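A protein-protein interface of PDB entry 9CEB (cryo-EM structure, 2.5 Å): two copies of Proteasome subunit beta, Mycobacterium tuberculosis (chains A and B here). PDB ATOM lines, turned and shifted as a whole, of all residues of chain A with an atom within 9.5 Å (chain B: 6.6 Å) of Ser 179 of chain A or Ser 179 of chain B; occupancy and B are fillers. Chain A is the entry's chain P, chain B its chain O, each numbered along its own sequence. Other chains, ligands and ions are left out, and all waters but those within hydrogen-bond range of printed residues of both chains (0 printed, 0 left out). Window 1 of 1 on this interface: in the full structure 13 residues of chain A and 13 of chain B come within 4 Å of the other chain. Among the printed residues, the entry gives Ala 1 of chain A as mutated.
The guanidinium group (NH1) of Arg 19 of chain A sits at hydrogen-bond distance from the backbone carbonyl oxygen (O) of Ser 179 of chain A (2.7 Å). The side-chain carboxylate (OD1) of Asp 178 of chain B is in hydrogen-bond range of the backbone NH (N) of Ala 180 of chain B. NH1 of Arg 19 of chain B sits at hydrogen-bond distance from O of Ser 179 of chain B (2.7 Å). OD2 of Asp 178 of chain A sits at hydrogen-bond distance from OG1 of Thr 181 of chain A (2.7 Å). The side-chain carboxylate (OD2) of Asp 178 of chain A sits at hydrogen-bond distance from the side-chain hydroxyl (OG) of Ser 141 of chain A.
Printed residues of chain A within 4 Å of Ser 179 of chain B: Asn 24 and Ser 179. Asp 178 of chain B touches one residue of chain A. Ala 180 of chain B touches just one residue of chain A: Asn 24. Of the printed residues of chain B, Asp 178 of chain A touches Asn 24 and Ile 26. Printed residues of chain B within 4 Å of Asp 176 of chain A: Ile 26. Of the printed residues of chain A, Ile 26 of chain B touches Asp 176 (3.8 Å), Asp 177 (3.4 Å), Asp 178 (3.99 Å) and Ser 179 (3.9 Å). Printed residues of chain B within 4 Å of Asp 177 of chain A: Ile 26 (3.4 Å). Printed residues of chain A within 4 Å of Asn 24 of chain B: Asp 178, Ser 179 and Ala 180. Thr 2 of chain A touches none of the printed residues of chain B. Ala 174 of chain B touches none of the printed residues of chain A. The nearest printed residue of chain A that does not touch Asp 177 of chain B is Arg 29 of chain A (4.2 Å).
Asn 24 of chain A touches Ser 179 of chain B, and with the chains exchanged Ser 179 of chain A touches Asn 24 of chain B. Asn 24 of chain A touches Ala 180 of chain B, and with the chains exchanged Ala 180 of chain A touches Asn 24 of chain B. Asp 178 of chain A touches Ile 26 of chain B, but with the chains exchanged Ile 26 of chain A does not touch Asp 178 of chain B (4.1 Å). Ser 179 of chain A touches Ile 26 of chain B, but with the chains exchanged Ile 26 of chain A does not touch Ser 179 of chain B (4.1 Å). Positions printed for both chains: 19, 21, 23, 24, 25, 26, 174, 175, 176, 177, 178, 179, 180, 181 and 182.
OD1 of Asn 24 of chain A touches N of Ala 180 of chain B, 3.8 Å away. CA of Met 25 of chain A touches O of Asp 177 of chain B (3.9 Å). Ile 26 of chain A touches Asp 176 of chain B (CD1 to O, 3.7 Å). Ile 26 of chain B touches Asp 176 of chain A (CD1 to O, 3.8 Å). Ile 26 of chain B touches Asp 178 of chain A (CD1 to C, 3.99 Å). N of Ser 179 of chain A touches CD1 of Ile 26 of chain B, 3.9 Å away. Ser 179 of chain B touches Ser 179 of chain A (OG to OG, 3.8 Å). OD1 of Asn 24 of chain B touches CB of Ala 180 of chain A, 3.996 Å away.
N of Ile 26 of chain B sits at hydrogen-bond distance from O of Asp 177 of chain A (3.4 Å). The side-chain carboxylate (OD2) of Asp 176 of chain B is in salt-bridge range of the guanidinium group (NH2) of Arg 29 of chain A, at 3.7 Å. The backbone carbonyl oxygen (O) of Asn 24 of chain A lies within hydrogen-bond range of the backbone NH (N) of Ser 179 of chain B (2.7 Å). O of Asn 24 of chain B lies close to OD1 of Asp 178 of chain A. The backbone carbonyl oxygen (O) of Asn 24 of chain B is in hydrogen-bond range of the backbone NH (N) of Ser 179 of chain A (3.0 Å). The backbone carbonyl oxygen (O) of Asn 24 of chain A sits close to the side-chain carboxylate (OD1) of Asp 178 of chain B (3.0 Å). The backbone carbonyl oxygen (O) of Asp 177 of chain B is in hydrogen-bond range of the backbone NH (N) of Ile 26 of chain A (3.3 Å).
Of the 15 printed residues of chain B, 7 touch a printed residue of chain A. Hydrophobic or aromatic side chains of chain B that line the printed part of chain A: Ile 26 and Ala 180. Of the 28 printed residues of chain A, 9 touch a printed residue of chain B. Hydrophobic or aromatic side chains of chain A within 4 Å of the printed part of chain B: Ile 26 and Ala 180. Among the printed residues, 15 pairs touch across the chains. Among the printed residues, Asp or Glu carboxylates within 4 Å of a Lys or Arg side-chain nitrogen of the other chain: Arg 29 of chain A with Asp 176 of chain B.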
ATOM      1  N   ALA A   1      22.395  -8.859   5.924  1.00  0.00           N
ATOM      2  CA  ALA A   1      23.122  -7.802   5.244  1.00  0.00           C
ATOM      3  C   ALA A   1      22.330  -6.507   5.263  1.00  0.00           C
ATOM      4  O   ALA A   1      21.143  -6.512   4.989  1.00  0.00           O
ATOM      5  CB  ALA A   1      23.432  -8.220   3.817  1.00  0.00           C
ATOM      6  N   THR A   2      22.982  -5.398   5.599  1.00  0.00           N
ATOM      7  CA  THR A   2      22.317  -4.104   5.649  1.00  0.00           C
ATOM      8  C   THR A   2      23.299  -3.026   5.215  1.00  0.00           C
ATOM      9  O   THR A   2      24.454  -3.028   5.637  1.00  0.00           O
ATOM     10  CB  THR A   2      21.758  -3.797   7.061  1.00  0.00           C
ATOM     11  OG1 THR A   2      21.065  -4.941   7.559  1.00  0.00           O
ATOM     12  CG2 THR A   2      20.791  -2.608   7.036  1.00  0.00           C
ATOM     13  N   ASP A  17      27.466  -3.691   6.541  1.00  0.00           N
ATOM     14  CA  ASP A  17      28.019  -4.724   7.410  1.00  0.00           C
ATOM     15  C   ASP A  17      28.885  -5.706   6.607  1.00  0.00           C
ATOM     16  O   ASP A  17      29.064  -5.571   5.397  1.00  0.00           O
ATOM     17  CB  ASP A  17      26.900  -5.451   8.166  1.00  0.00           C
ATOM     18  CG  ASP A  17      26.164  -6.479   7.310  1.00  0.00           C
ATOM     19  OD1 ASP A  17      25.636  -6.113   6.247  1.00  0.00           O
ATOM     20  OD2 ASP A  17      26.114  -7.664   7.710  1.00  0.00           O
ATOM     21  N   ARG A  19      28.828  -9.443   6.865  1.00  0.00           N
ATOM     22  CA  ARG A  19      28.452 -10.846   6.989  1.00  0.00           C
ATOM     23  C   ARG A  19      27.823 -11.375   5.704  1.00  0.00           C
ATOM     24  O   ARG A  19      27.066 -10.670   5.033  1.00  0.00           O
ATOM     25  CB  ARG A  19      27.479 -11.035   8.149  1.00  0.00           C
ATOM     26  CG  ARG A  19      27.034 -12.465   8.343  1.00  0.00           C
ATOM     27  CD  ARG A  19      26.211 -12.638   9.574  1.00  0.00           C
ATOM     28  NE  ARG A  19      27.052 -12.986  10.710  1.00  0.00           N
ATOM     29  CZ  ARG A  19      26.629 -13.027  11.964  1.00  0.00           C
ATOM     30  NH1 ARG A  19      25.357 -12.871  12.270  1.00  0.00           N
ATOM     31  NH2 ARG A  19      27.507 -13.245  12.934  1.00  0.00           N
ATOM     32  N   SER A  20      28.157 -12.612   5.354  1.00  0.00           N
ATOM     33  CA  SER A  20      27.457 -13.351   4.312  1.00  0.00           C
ATOM     34  C   SER A  20      27.019 -14.696   4.878  1.00  0.00           C
ATOM     35  O   SER A  20      27.734 -15.303   5.677  1.00  0.00           O
ATOM     36  CB  SER A  20      28.328 -13.522   3.054  1.00  0.00           C
ATOM     37  OG  SER A  20      29.287 -14.546   3.194  1.00  0.00           O
ATOM     38  N   THR A  21      25.818 -15.134   4.511  1.00  0.00           N
ATOM     39  CA  THR A  21      25.206 -16.325   5.086  1.00  0.00           C
ATOM     40  C   THR A  21      24.689 -17.237   3.985  1.00  0.00           C
ATOM     41  O   THR A  21      24.303 -16.783   2.906  1.00  0.00           O
ATOM     42  CB  THR A  21      24.030 -15.982   6.049  1.00  0.00           C
ATOM     43  OG1 THR A  21      23.300 -14.852   5.555  1.00  0.00           O
ATOM     44  CG2 THR A  21      24.527 -15.696   7.471  1.00  0.00           C
ATOM     45  N   GLN A  22      24.693 -18.534   4.273  1.00  0.00           N
ATOM     46  CA  GLN A  22      24.076 -19.566   3.440  1.00  0.00           C
ATOM     47  C   GLN A  22      23.061 -20.289   4.316  1.00  0.00           C
ATOM     48  O   GLN A  22      23.364 -21.326   4.906  1.00  0.00           O
ATOM     49  CB  GLN A  22      25.111 -20.528   2.885  1.00  0.00           C
ATOM     50  CG  GLN A  22      25.767 -20.062   1.612  1.00  0.00           C
ATOM     51  CD  GLN A  22      27.037 -20.819   1.299  1.00  0.00           C
ATOM     52  OE1 GLN A  22      27.504 -21.630   2.096  1.00  0.00           O
ATOM     53  NE2 GLN A  22      27.610 -20.554   0.133  1.00  0.00           N
ATOM     54  N   GLY A  23      21.850 -19.750   4.389  1.00  0.00           N
ATOM     55  CA  GLY A  23      20.873 -20.242   5.338  1.00  0.00           C
ATOM     56  C   GLY A  23      21.149 -19.730   6.736  1.00  0.00           C
ATOM     57  O   GLY A  23      21.161 -18.520   6.964  1.00  0.00           O
ATOM     58  N   ASN A  24      21.380 -20.638   7.679  1.00  0.00           N
ATOM     59  CA  ASN A  24      21.780 -20.279   9.031  1.00  0.00           C
ATOM     60  C   ASN A  24      23.278 -20.394   9.248  1.00  0.00           C
ATOM     61  O   ASN A  24      23.749 -20.141  10.356  1.00  0.00           O
ATOM     62  CB  ASN A  24      21.041 -21.151  10.049  1.00  0.00           C
ATOM     63  CG  ASN A  24      19.806 -20.480  10.603  1.00  0.00           C
ATOM     64  OD1 ASN A  24      19.812 -19.285  10.903  1.00  0.00           O
ATOM     65  ND2 ASN A  24      18.729 -21.242  10.724  1.00  0.00           N
ATOM     66  N   MET A  25      24.036 -20.756   8.223  1.00  0.00           N
ATOM     67  CA  MET A  25      25.472 -20.954   8.337  1.00  0.00           C
ATOM     68  C   MET A  25      26.215 -19.699   7.907  1.00  0.00           C
ATOM     69  O   MET A  25      25.948 -19.155   6.834  1.00  0.00           O
ATOM     70  CB  MET A  25      25.918 -22.148   7.494  1.00  0.00           C
ATOM     71  CG  MET A  25      25.726 -23.479   8.181  1.00  0.00           C
ATOM     72  SD  MET A  25      26.411 -24.833   7.222  1.00  0.00           S
ATOM     73  CE  MET A  25      28.104 -24.277   7.057  1.00  0.00           C
ATOM     74  N   ILE A  26      27.145 -19.244   8.748  1.00  0.00           N
ATOM     75  CA  ILE A  26      27.973 -18.093   8.408  1.00  0.00           C
ATOM     76  C   ILE A  26      29.032 -18.512   7.398  1.00  0.00           C
ATOM     77  O   ILE A  26      29.847 -19.407   7.652  1.00  0.00           O
ATOM     78  CB  ILE A  26      28.599 -17.471   9.666  1.00  0.00           C
ATOM     79  CG1 ILE A  26      27.509 -16.958  10.612  1.00  0.00           C
ATOM     80  CG2 ILE A  26      29.582 -16.369   9.312  1.00  0.00           C
ATOM     81  CD1 ILE A  26      27.778 -17.202  12.066  1.00  0.00           C
ATOM     82  N   SER A  27      29.025 -17.860   6.236  1.00  0.00           N
ATOM     83  CA  SER A  27      29.939 -18.197   5.160  1.00  0.00           C
ATOM     84  C   SER A  27      31.026 -17.157   4.928  1.00  0.00           C
ATOM     85  O   SER A  27      32.038 -17.484   4.307  1.00  0.00           O
ATOM     86  CB  SER A  27      29.156 -18.430   3.859  1.00  0.00           C
ATOM     87  OG  SER A  27      29.046 -17.255   3.087  1.00  0.00           O
ATOM     88  N   GLY A  28      30.859 -15.938   5.415  1.00  0.00           N
ATOM     89  CA  GLY A  28      31.889 -14.924   5.275  1.00  0.00           C
ATOM     90  C   GLY A  28      31.836 -13.939   6.416  1.00  0.00           C
ATOM     91  O   GLY A  28      30.766 -13.631   6.941  1.00  0.00           O
ATOM     92  N   ARG A  29      33.009 -13.437   6.799  1.00  0.00           N
ATOM     93  CA  ARG A  29      33.129 -12.480   7.889  1.00  0.00           C
ATOM     94  C   ARG A  29      33.779 -11.168   7.473  1.00  0.00           C
ATOM     95  O   ARG A  29      33.910 -10.273   8.308  1.00  0.00           O
ATOM     96  CB  ARG A  29      33.940 -13.084   9.046  1.00  0.00           C
ATOM     97  CG  ARG A  29      33.549 -14.476   9.448  1.00  0.00           C
ATOM     98  CD  ARG A  29      34.535 -15.044  10.442  1.00  0.00           C
ATOM     99  NE  ARG A  29      34.293 -16.451  10.740  1.00  0.00           N
ATOM    100  CZ  ARG A  29      33.246 -16.918  11.404  1.00  0.00           C
ATOM    101  NH1 ARG A  29      32.376 -16.112  11.986  1.00  0.00           N
ATOM    102  NH2 ARG A  29      33.078 -18.230  11.501  1.00  0.00           N
ATOM    103  N   SER A 141      18.149  -7.075   4.866  1.00  0.00           N
ATOM    104  CA  SER A 141      17.246  -7.811   5.749  1.00  0.00           C
ATOM    105  C   SER A 141      17.084  -7.158   7.118  1.00  0.00           C
ATOM    106  O   SER A 141      16.138  -7.490   7.837  1.00  0.00           O
ATOM    107  CB  SER A 141      17.724  -9.250   5.928  1.00  0.00           C
ATOM    108  OG  SER A 141      19.100  -9.305   6.244  1.00  0.00           O
ATOM    109  N   GLY A 142      17.974  -6.248   7.498  1.00  0.00           N
ATOM    110  CA  GLY A 142      17.806  -5.506   8.729  1.00  0.00           C
ATOM    111  C   GLY A 142      17.483  -4.049   8.489  1.00  0.00           C
ATOM    112  O   GLY A 142      17.725  -3.209   9.353  1.00  0.00           O
ATOM    113  N   PHE A 145      14.831  -2.235  11.044  1.00  0.00           N
ATOM    114  CA  PHE A 145      15.396  -1.870  12.340  1.00  0.00           C
ATOM    115  C   PHE A 145      16.336  -0.678  12.233  1.00  0.00           C
ATOM    116  O   PHE A 145      16.322   0.213  13.091  1.00  0.00           O
ATOM    117  CB  PHE A 145      16.126  -3.062  12.957  1.00  0.00           C
ATOM    118  CG  PHE A 145      15.304  -4.305  13.035  1.00  0.00           C
ATOM    119  CD1 PHE A 145      14.227  -4.380  13.900  1.00  0.00           C
ATOM    120  CD2 PHE A 145      15.599  -5.406  12.245  1.00  0.00           C
ATOM    121  CE1 PHE A 145      13.464  -5.518  13.982  1.00  0.00           C
ATOM    122  CE2 PHE A 145      14.835  -6.549  12.319  1.00  0.00           C
ATOM    123  CZ  PHE A 145      13.763  -6.602  13.193  1.00  0.00           C
ATOM    124  N   ASP A 173      22.237  -1.482  15.720  1.00  0.00           N
ATOM    125  CA  ASP A 173      20.864  -1.866  16.058  1.00  0.00           C
ATOM    126  C   ASP A 173      20.307  -2.924  15.108  1.00  0.00           C
ATOM    127  O   ASP A 173      19.618  -3.863  15.540  1.00  0.00           O
ATOM    128  CB  ASP A 173      19.963  -0.637  16.064  1.00  0.00           C
ATOM    129  CG  ASP A 173      20.102   0.172  17.318  1.00  0.00           C
ATOM    130  OD1 ASP A 173      20.060  -0.430  18.405  1.00  0.00           O
ATOM    131  OD2 ASP A 173      20.262   1.403  17.220  1.00  0.00           O
ATOM    132  N   ALA A 174      20.587  -2.785  13.809  1.00  0.00           N
ATOM    133  CA  ALA A 174      20.178  -3.819  12.863  1.00  0.00           C
ATOM    134  C   ALA A 174      20.797  -5.170  13.209  1.00  0.00           C
ATOM    135  O   ALA A 174      20.118  -6.199  13.143  1.00  0.00           O
ATOM    136  CB  ALA A 174      20.536  -3.409  11.440  1.00  0.00           C
ATOM    137  N   ALA A 175      22.083  -5.193  13.577  1.00  0.00           N
ATOM    138  CA  ALA A 175      22.710  -6.458  13.955  1.00  0.00           C
ATOM    139  C   ALA A 175      22.112  -7.007  15.242  1.00  0.00           C
ATOM    140  O   ALA A 175      22.005  -8.224  15.417  1.00  0.00           O
ATOM    141  CB  ALA A 175      24.213  -6.286  14.110  1.00  0.00           C
ATOM    142  N   ASP A 176      21.737  -6.119  16.156  1.00  0.00           N
ATOM    143  CA  ASP A 176      21.137  -6.549  17.407  1.00  0.00           C
ATOM    144  C   ASP A 176      19.785  -7.210  17.189  1.00  0.00           C
ATOM    145  O   ASP A 176      19.382  -8.067  17.979  1.00  0.00           O
ATOM    146  CB  ASP A 176      21.000  -5.350  18.330  1.00  0.00           C
ATOM    147  CG  ASP A 176      20.942  -5.738  19.768  1.00  0.00           C
ATOM    148  OD1 ASP A 176      21.833  -6.486  20.213  1.00  0.00           O
ATOM    149  OD2 ASP A 176      20.003  -5.294  20.450  1.00  0.00           O
ATOM    150  N   ASP A 177      19.069  -6.838  16.127  1.00  0.00           N
ATOM    151  CA  ASP A 177      17.738  -7.389  15.920  1.00  0.00           C
ATOM    152  C   ASP A 177      17.663  -8.513  14.886  1.00  0.00           C
ATOM    153  O   ASP A 177      16.753  -9.336  14.974  1.00  0.00           O
ATOM    154  CB  ASP A 177      16.772  -6.272  15.526  1.00  0.00           C
ATOM    155  CG  ASP A 177      16.469  -5.327  16.680  1.00  0.00           C
ATOM    156  OD1 ASP A 177      15.844  -5.772  17.663  1.00  0.00           O
ATOM    157  OD2 ASP A 177      16.850  -4.136  16.604  1.00  0.00           O
ATOM    158  N   ASP A 178      18.585  -8.589  13.923  1.00  0.00           N
ATOM    159  CA  ASP A 178      18.504  -9.557  12.831  1.00  0.00           C
ATOM    160  C   ASP A 178      19.810 -10.340  12.760  1.00  0.00           C
ATOM    161  O   ASP A 178      20.893  -9.755  12.798  1.00  0.00           O
ATOM    162  CB  ASP A 178      18.212  -8.848  11.477  1.00  0.00           C
ATOM    163  CG  ASP A 178      18.693  -9.636  10.259  1.00  0.00           C
ATOM    164  OD1 ASP A 178      18.407 -10.847  10.171  1.00  0.00           O
ATOM    165  OD2 ASP A 178      19.349  -9.047   9.379  1.00  0.00           O
ATOM    166  N   SER A 179      19.703 -11.665  12.649  1.00  0.00           N
ATOM    167  CA  SER A 179      20.869 -12.539  12.736  1.00  0.00           C
ATOM    168  C   SER A 179      21.635 -12.677  11.423  1.00  0.00           C
ATOM    169  O   SER A 179      22.770 -13.154  11.442  1.00  0.00           O
ATOM    170  CB  SER A 179      20.458 -13.926  13.250  1.00  0.00           C
ATOM    171  OG  SER A 179      19.833 -14.702  12.247  1.00  0.00           O
ATOM    172  N   ALA A 180      21.065 -12.263  10.294  1.00  0.00           N
ATOM    173  CA  ALA A 180      21.809 -12.258   9.043  1.00  0.00           C
ATOM    174  C   ALA A 180      22.753 -11.069   8.926  1.00  0.00           C
ATOM    175  O   ALA A 180      23.590 -11.050   8.019  1.00  0.00           O
ATOM    176  CB  ALA A 180      20.852 -12.284   7.855  1.00  0.00           C
ATOM    177  N   THR A 181      22.640 -10.089   9.816  1.00  0.00           N
ATOM    178  CA  THR A 181      23.532  -8.939   9.871  1.00  0.00           C
ATOM    179  C   THR A 181      24.562  -9.158  10.973  1.00  0.00           C
ATOM    180  O   THR A 181      24.215  -9.567  12.082  1.00  0.00           O
ATOM    181  CB  THR A 181      22.732  -7.651  10.124  1.00  0.00           C
ATOM    182  OG1 THR A 181      21.633  -7.581   9.210  1.00  0.00           O
ATOM    183  CG2 THR A 181      23.599  -6.408   9.985  1.00  0.00           C
ATOM    184  N   GLY A 182      25.823  -8.900  10.660  1.00  0.00           N
ATOM    185  CA  GLY A 182      26.907  -9.068  11.607  1.00  0.00           C
ATOM    186  C   GLY A 182      27.217  -7.778  12.347  1.00  0.00           C
ATOM    187  O   GLY A 182      27.247  -6.703  11.754  1.00  0.00           O
ATOM    188  N   GLY A 183      27.433  -7.902  13.653  1.00  0.00           N
ATOM    189  CA  GLY A 183      27.832  -6.783  14.471  1.00  0.00           C
ATOM    190  C   GLY A 183      29.333  -6.592  14.488  1.00  0.00           C
ATOM    191  O   GLY A 183      30.080  -7.356  13.874  1.00  0.00           O
ATOM    192  N   ARG B  19      19.299 -18.742  22.650  1.00  0.00           N
ATOM    193  CA  ARG B  19      18.686 -18.005  21.553  1.00  0.00           C
ATOM    194  C   ARG B  19      17.455 -18.724  21.010  1.00  0.00           C
ATOM    195  O   ARG B  19      17.431 -19.953  20.915  1.00  0.00           O
ATOM    196  CB  ARG B  19      19.693 -17.795  20.425  1.00  0.00           C
ATOM    197  CG  ARG B  19      19.134 -17.040  19.243  1.00  0.00           C
ATOM    198  CD  ARG B  19      20.183 -16.718  18.232  1.00  0.00           C
ATOM    199  NE  ARG B  19      20.768 -15.413  18.497  1.00  0.00           N
ATOM    200  CZ  ARG B  19      21.839 -14.938  17.880  1.00  0.00           C
ATOM    201  NH1 ARG B  19      22.394 -15.577  16.870  1.00  0.00           N
ATOM    202  NH2 ARG B  19      22.356 -13.784  18.279  1.00  0.00           N
ATOM    203  N   THR B  21      14.744 -18.134  17.564  1.00  0.00           N
ATOM    204  CA  THR B  21      14.657 -17.414  16.299  1.00  0.00           C
ATOM    205  C   THR B  21      13.344 -17.730  15.601  1.00  0.00           C
ATOM    206  O   THR B  21      12.784 -18.818  15.753  1.00  0.00           O
ATOM    207  CB  THR B  21      15.834 -17.758  15.339  1.00  0.00           C
ATOM    208  OG1 THR B  21      16.186 -19.142  15.462  1.00  0.00           O
ATOM    209  CG2 THR B  21      17.065 -16.886  15.613  1.00  0.00           C
ATOM    210  N   GLY B  23      12.768 -17.513  11.839  1.00  0.00           N
ATOM    211  CA  GLY B  23      13.436 -17.232  10.585  1.00  0.00           C
ATOM    212  C   GLY B  23      14.809 -16.636  10.808  1.00  0.00           C
ATOM    213  O   GLY B  23      15.665 -17.264  11.434  1.00  0.00           O
ATOM    214  N   ASN B  24      15.034 -15.424  10.311  1.00  0.00           N
ATOM    215  CA  ASN B  24      16.264 -14.691  10.561  1.00  0.00           C
ATOM    216  C   ASN B  24      16.119 -13.665  11.672  1.00  0.00           C
ATOM    217  O   ASN B  24      17.080 -12.958  11.970  1.00  0.00           O
ATOM    218  CB  ASN B  24      16.736 -13.999   9.278  1.00  0.00           C
ATOM    219  CG  ASN B  24      17.772 -14.805   8.531  1.00  0.00           C
ATOM    220  OD1 ASN B  24      18.679 -15.386   9.129  1.00  0.00           O
ATOM    221  ND2 ASN B  24      17.634 -14.860   7.215  1.00  0.00           N
ATOM    222  N   MET B  25      14.953 -13.577  12.296  1.00  0.00           N
ATOM    223  CA  MET B  25      14.688 -12.590  13.332  1.00  0.00           C
ATOM    224  C   MET B  25      14.906 -13.198  14.709  1.00  0.00           C
ATOM    225  O   MET B  25      14.381 -14.273  15.004  1.00  0.00           O
ATOM    226  CB  MET B  25      13.263 -12.054  13.211  1.00  0.00           C
ATOM    227  CG  MET B  25      13.116 -10.951  12.189  1.00  0.00           C
ATOM    228  SD  MET B  25      11.466 -10.244  12.197  1.00  0.00           S
ATOM    229  CE  MET B  25      11.349  -9.741  13.911  1.00  0.00           C
ATOM    230  N   ILE B  26      15.683 -12.508  15.544  1.00  0.00           N
ATOM    231  CA  ILE B  26      15.902 -12.954  16.914  1.00  0.00           C
ATOM    232  C   ILE B  26      14.665 -12.654  17.750  1.00  0.00           C
ATOM    233  O   ILE B  26      14.235 -11.501  17.871  1.00  0.00           O
ATOM    234  CB  ILE B  26      17.164 -12.311  17.512  1.00  0.00           C
ATOM    235  CG1 ILE B  26      18.406 -12.722  16.717  1.00  0.00           C
ATOM    236  CG2 ILE B  26      17.317 -12.647  18.985  1.00  0.00           C
ATOM    237  CD1 ILE B  26      19.408 -11.626  16.511  1.00  0.00           C
ATOM    238  N   ALA B 174      30.065 -23.715  18.200  1.00  0.00           N
ATOM    239  CA  ALA B 174      28.793 -23.811  17.492  1.00  0.00           C
ATOM    240  C   ALA B 174      28.218 -22.430  17.188  1.00  0.00           C
ATOM    241  O   ALA B 174      27.710 -22.197  16.085  1.00  0.00           O
ATOM    242  CB  ALA B 174      27.801 -24.644  18.292  1.00  0.00           C
ATOM    243  N   ALA B 175      28.282 -21.499  18.146  1.00  0.00           N
ATOM    244  CA  ALA B 175      27.780 -20.151  17.887  1.00  0.00           C
ATOM    245  C   ALA B 175      28.626 -19.438  16.844  1.00  0.00           C
ATOM    246  O   ALA B 175      28.112 -18.638  16.055  1.00  0.00           O
ATOM    247  CB  ALA B 175      27.743 -19.338  19.173  1.00  0.00           C
ATOM    248  N   ASP B 176      29.928 -19.705  16.840  1.00  0.00           N
ATOM    249  CA  ASP B 176      30.810 -19.088  15.866  1.00  0.00           C
ATOM    250  C   ASP B 176      30.500 -19.544  14.449  1.00  0.00           C
ATOM    251  O   ASP B 176      30.736 -18.799  13.495  1.00  0.00           O
ATOM    252  CB  ASP B 176      32.250 -19.412  16.225  1.00  0.00           C
ATOM    253  CG  ASP B 176      33.216 -18.416  15.678  1.00  0.00           C
ATOM    254  OD1 ASP B 176      33.010 -17.209  15.904  1.00  0.00           O
ATOM    255  OD2 ASP B 176      34.180 -18.845  15.021  1.00  0.00           O
ATOM    256  N   ASP B 177      29.966 -20.754  14.285  1.00  0.00           N
ATOM    257  CA  ASP B 177      29.720 -21.262  12.943  1.00  0.00           C
ATOM    258  C   ASP B 177      28.269 -21.164  12.475  1.00  0.00           C
ATOM    259  O   ASP B 177      28.040 -21.105  11.266  1.00  0.00           O
ATOM    260  CB  ASP B 177      30.186 -22.714  12.847  1.00  0.00           C
ATOM    261  CG  ASP B 177      31.701 -22.846  12.887  1.00  0.00           C
ATOM    262  OD1 ASP B 177      32.363 -22.379  11.937  1.00  0.00           O
ATOM    263  OD2 ASP B 177      32.236 -23.423  13.862  1.00  0.00           O
ATOM    264  N   ASP B 178      27.284 -21.128  13.375  1.00  0.00           N
ATOM    265  CA  ASP B 178      25.871 -21.161  12.999  1.00  0.00           C
ATOM    266  C   ASP B 178      25.154 -19.984  13.646  1.00  0.00           C
ATOM    267  O   ASP B 178      25.323 -19.726  14.839  1.00  0.00           O
ATOM    268  CB  ASP B 178      25.214 -22.507  13.421  1.00  0.00           C
ATOM    269  CG  ASP B 178      23.702 -22.410  13.625  1.00  0.00           C
ATOM    270  OD1 ASP B 178      23.008 -21.858  12.749  1.00  0.00           O
ATOM    271  OD2 ASP B 178      23.199 -22.894  14.658  1.00  0.00           O
ATOM    272  N   SER B 179      24.347 -19.273  12.858  1.00  0.00           N
ATOM    273  CA  SER B 179      23.731 -18.029  13.311  1.00  0.00           C
ATOM    274  C   SER B 179      22.455 -18.232  14.120  1.00  0.00           C
ATOM    275  O   SER B 179      22.009 -17.291  14.779  1.00  0.00           O
ATOM    276  CB  SER B 179      23.451 -17.107  12.115  1.00  0.00           C
ATOM    277  OG  SER B 179      22.313 -17.515  11.382  1.00  0.00           O
ATOM    278  N   ALA B 180      21.864 -19.424  14.109  1.00  0.00           N
ATOM    279  CA  ALA B 180      20.720 -19.695  14.968  1.00  0.00           C
ATOM    280  C   ALA B 180      21.122 -19.980  16.410  1.00  0.00           C
ATOM    281  O   ALA B 180      20.251 -20.021  17.282  1.00  0.00           O
ATOM    282  CB  ALA B 180      19.904 -20.859  14.415  1.00  0.00           C
ATOM    283  N   THR B 181      22.410 -20.171  16.675  1.00  0.00           N
ATOM    284  CA  THR B 181      22.939 -20.366  18.017  1.00  0.00           C
ATOM    285  C   THR B 181      23.536 -19.054  18.514  1.00  0.00           C
ATOM    286  O   THR B 181      24.272 -18.386  17.786  1.00  0.00           O
ATOM    287  CB  THR B 181      23.997 -21.481  18.022  1.00  0.00           C
ATOM    288  OG1 THR B 181      23.481 -22.634  17.350  1.00  0.00           O
ATOM    289  CG2 THR B 181      24.423 -21.853  19.434  1.00  0.00           C
ATOM    290  N   GLY B 182      23.207 -18.686  19.743  1.00  0.00           N
ATOM    291  CA  GLY B 182      23.698 -17.460  20.342  1.00  0.00           C
ATOM    292  C   GLY B 182      24.962 -17.693  21.151  1.00  0.00           C
ATOM    293  O   GLY B 182      25.070 -18.674  21.882  1.00  0.00           O
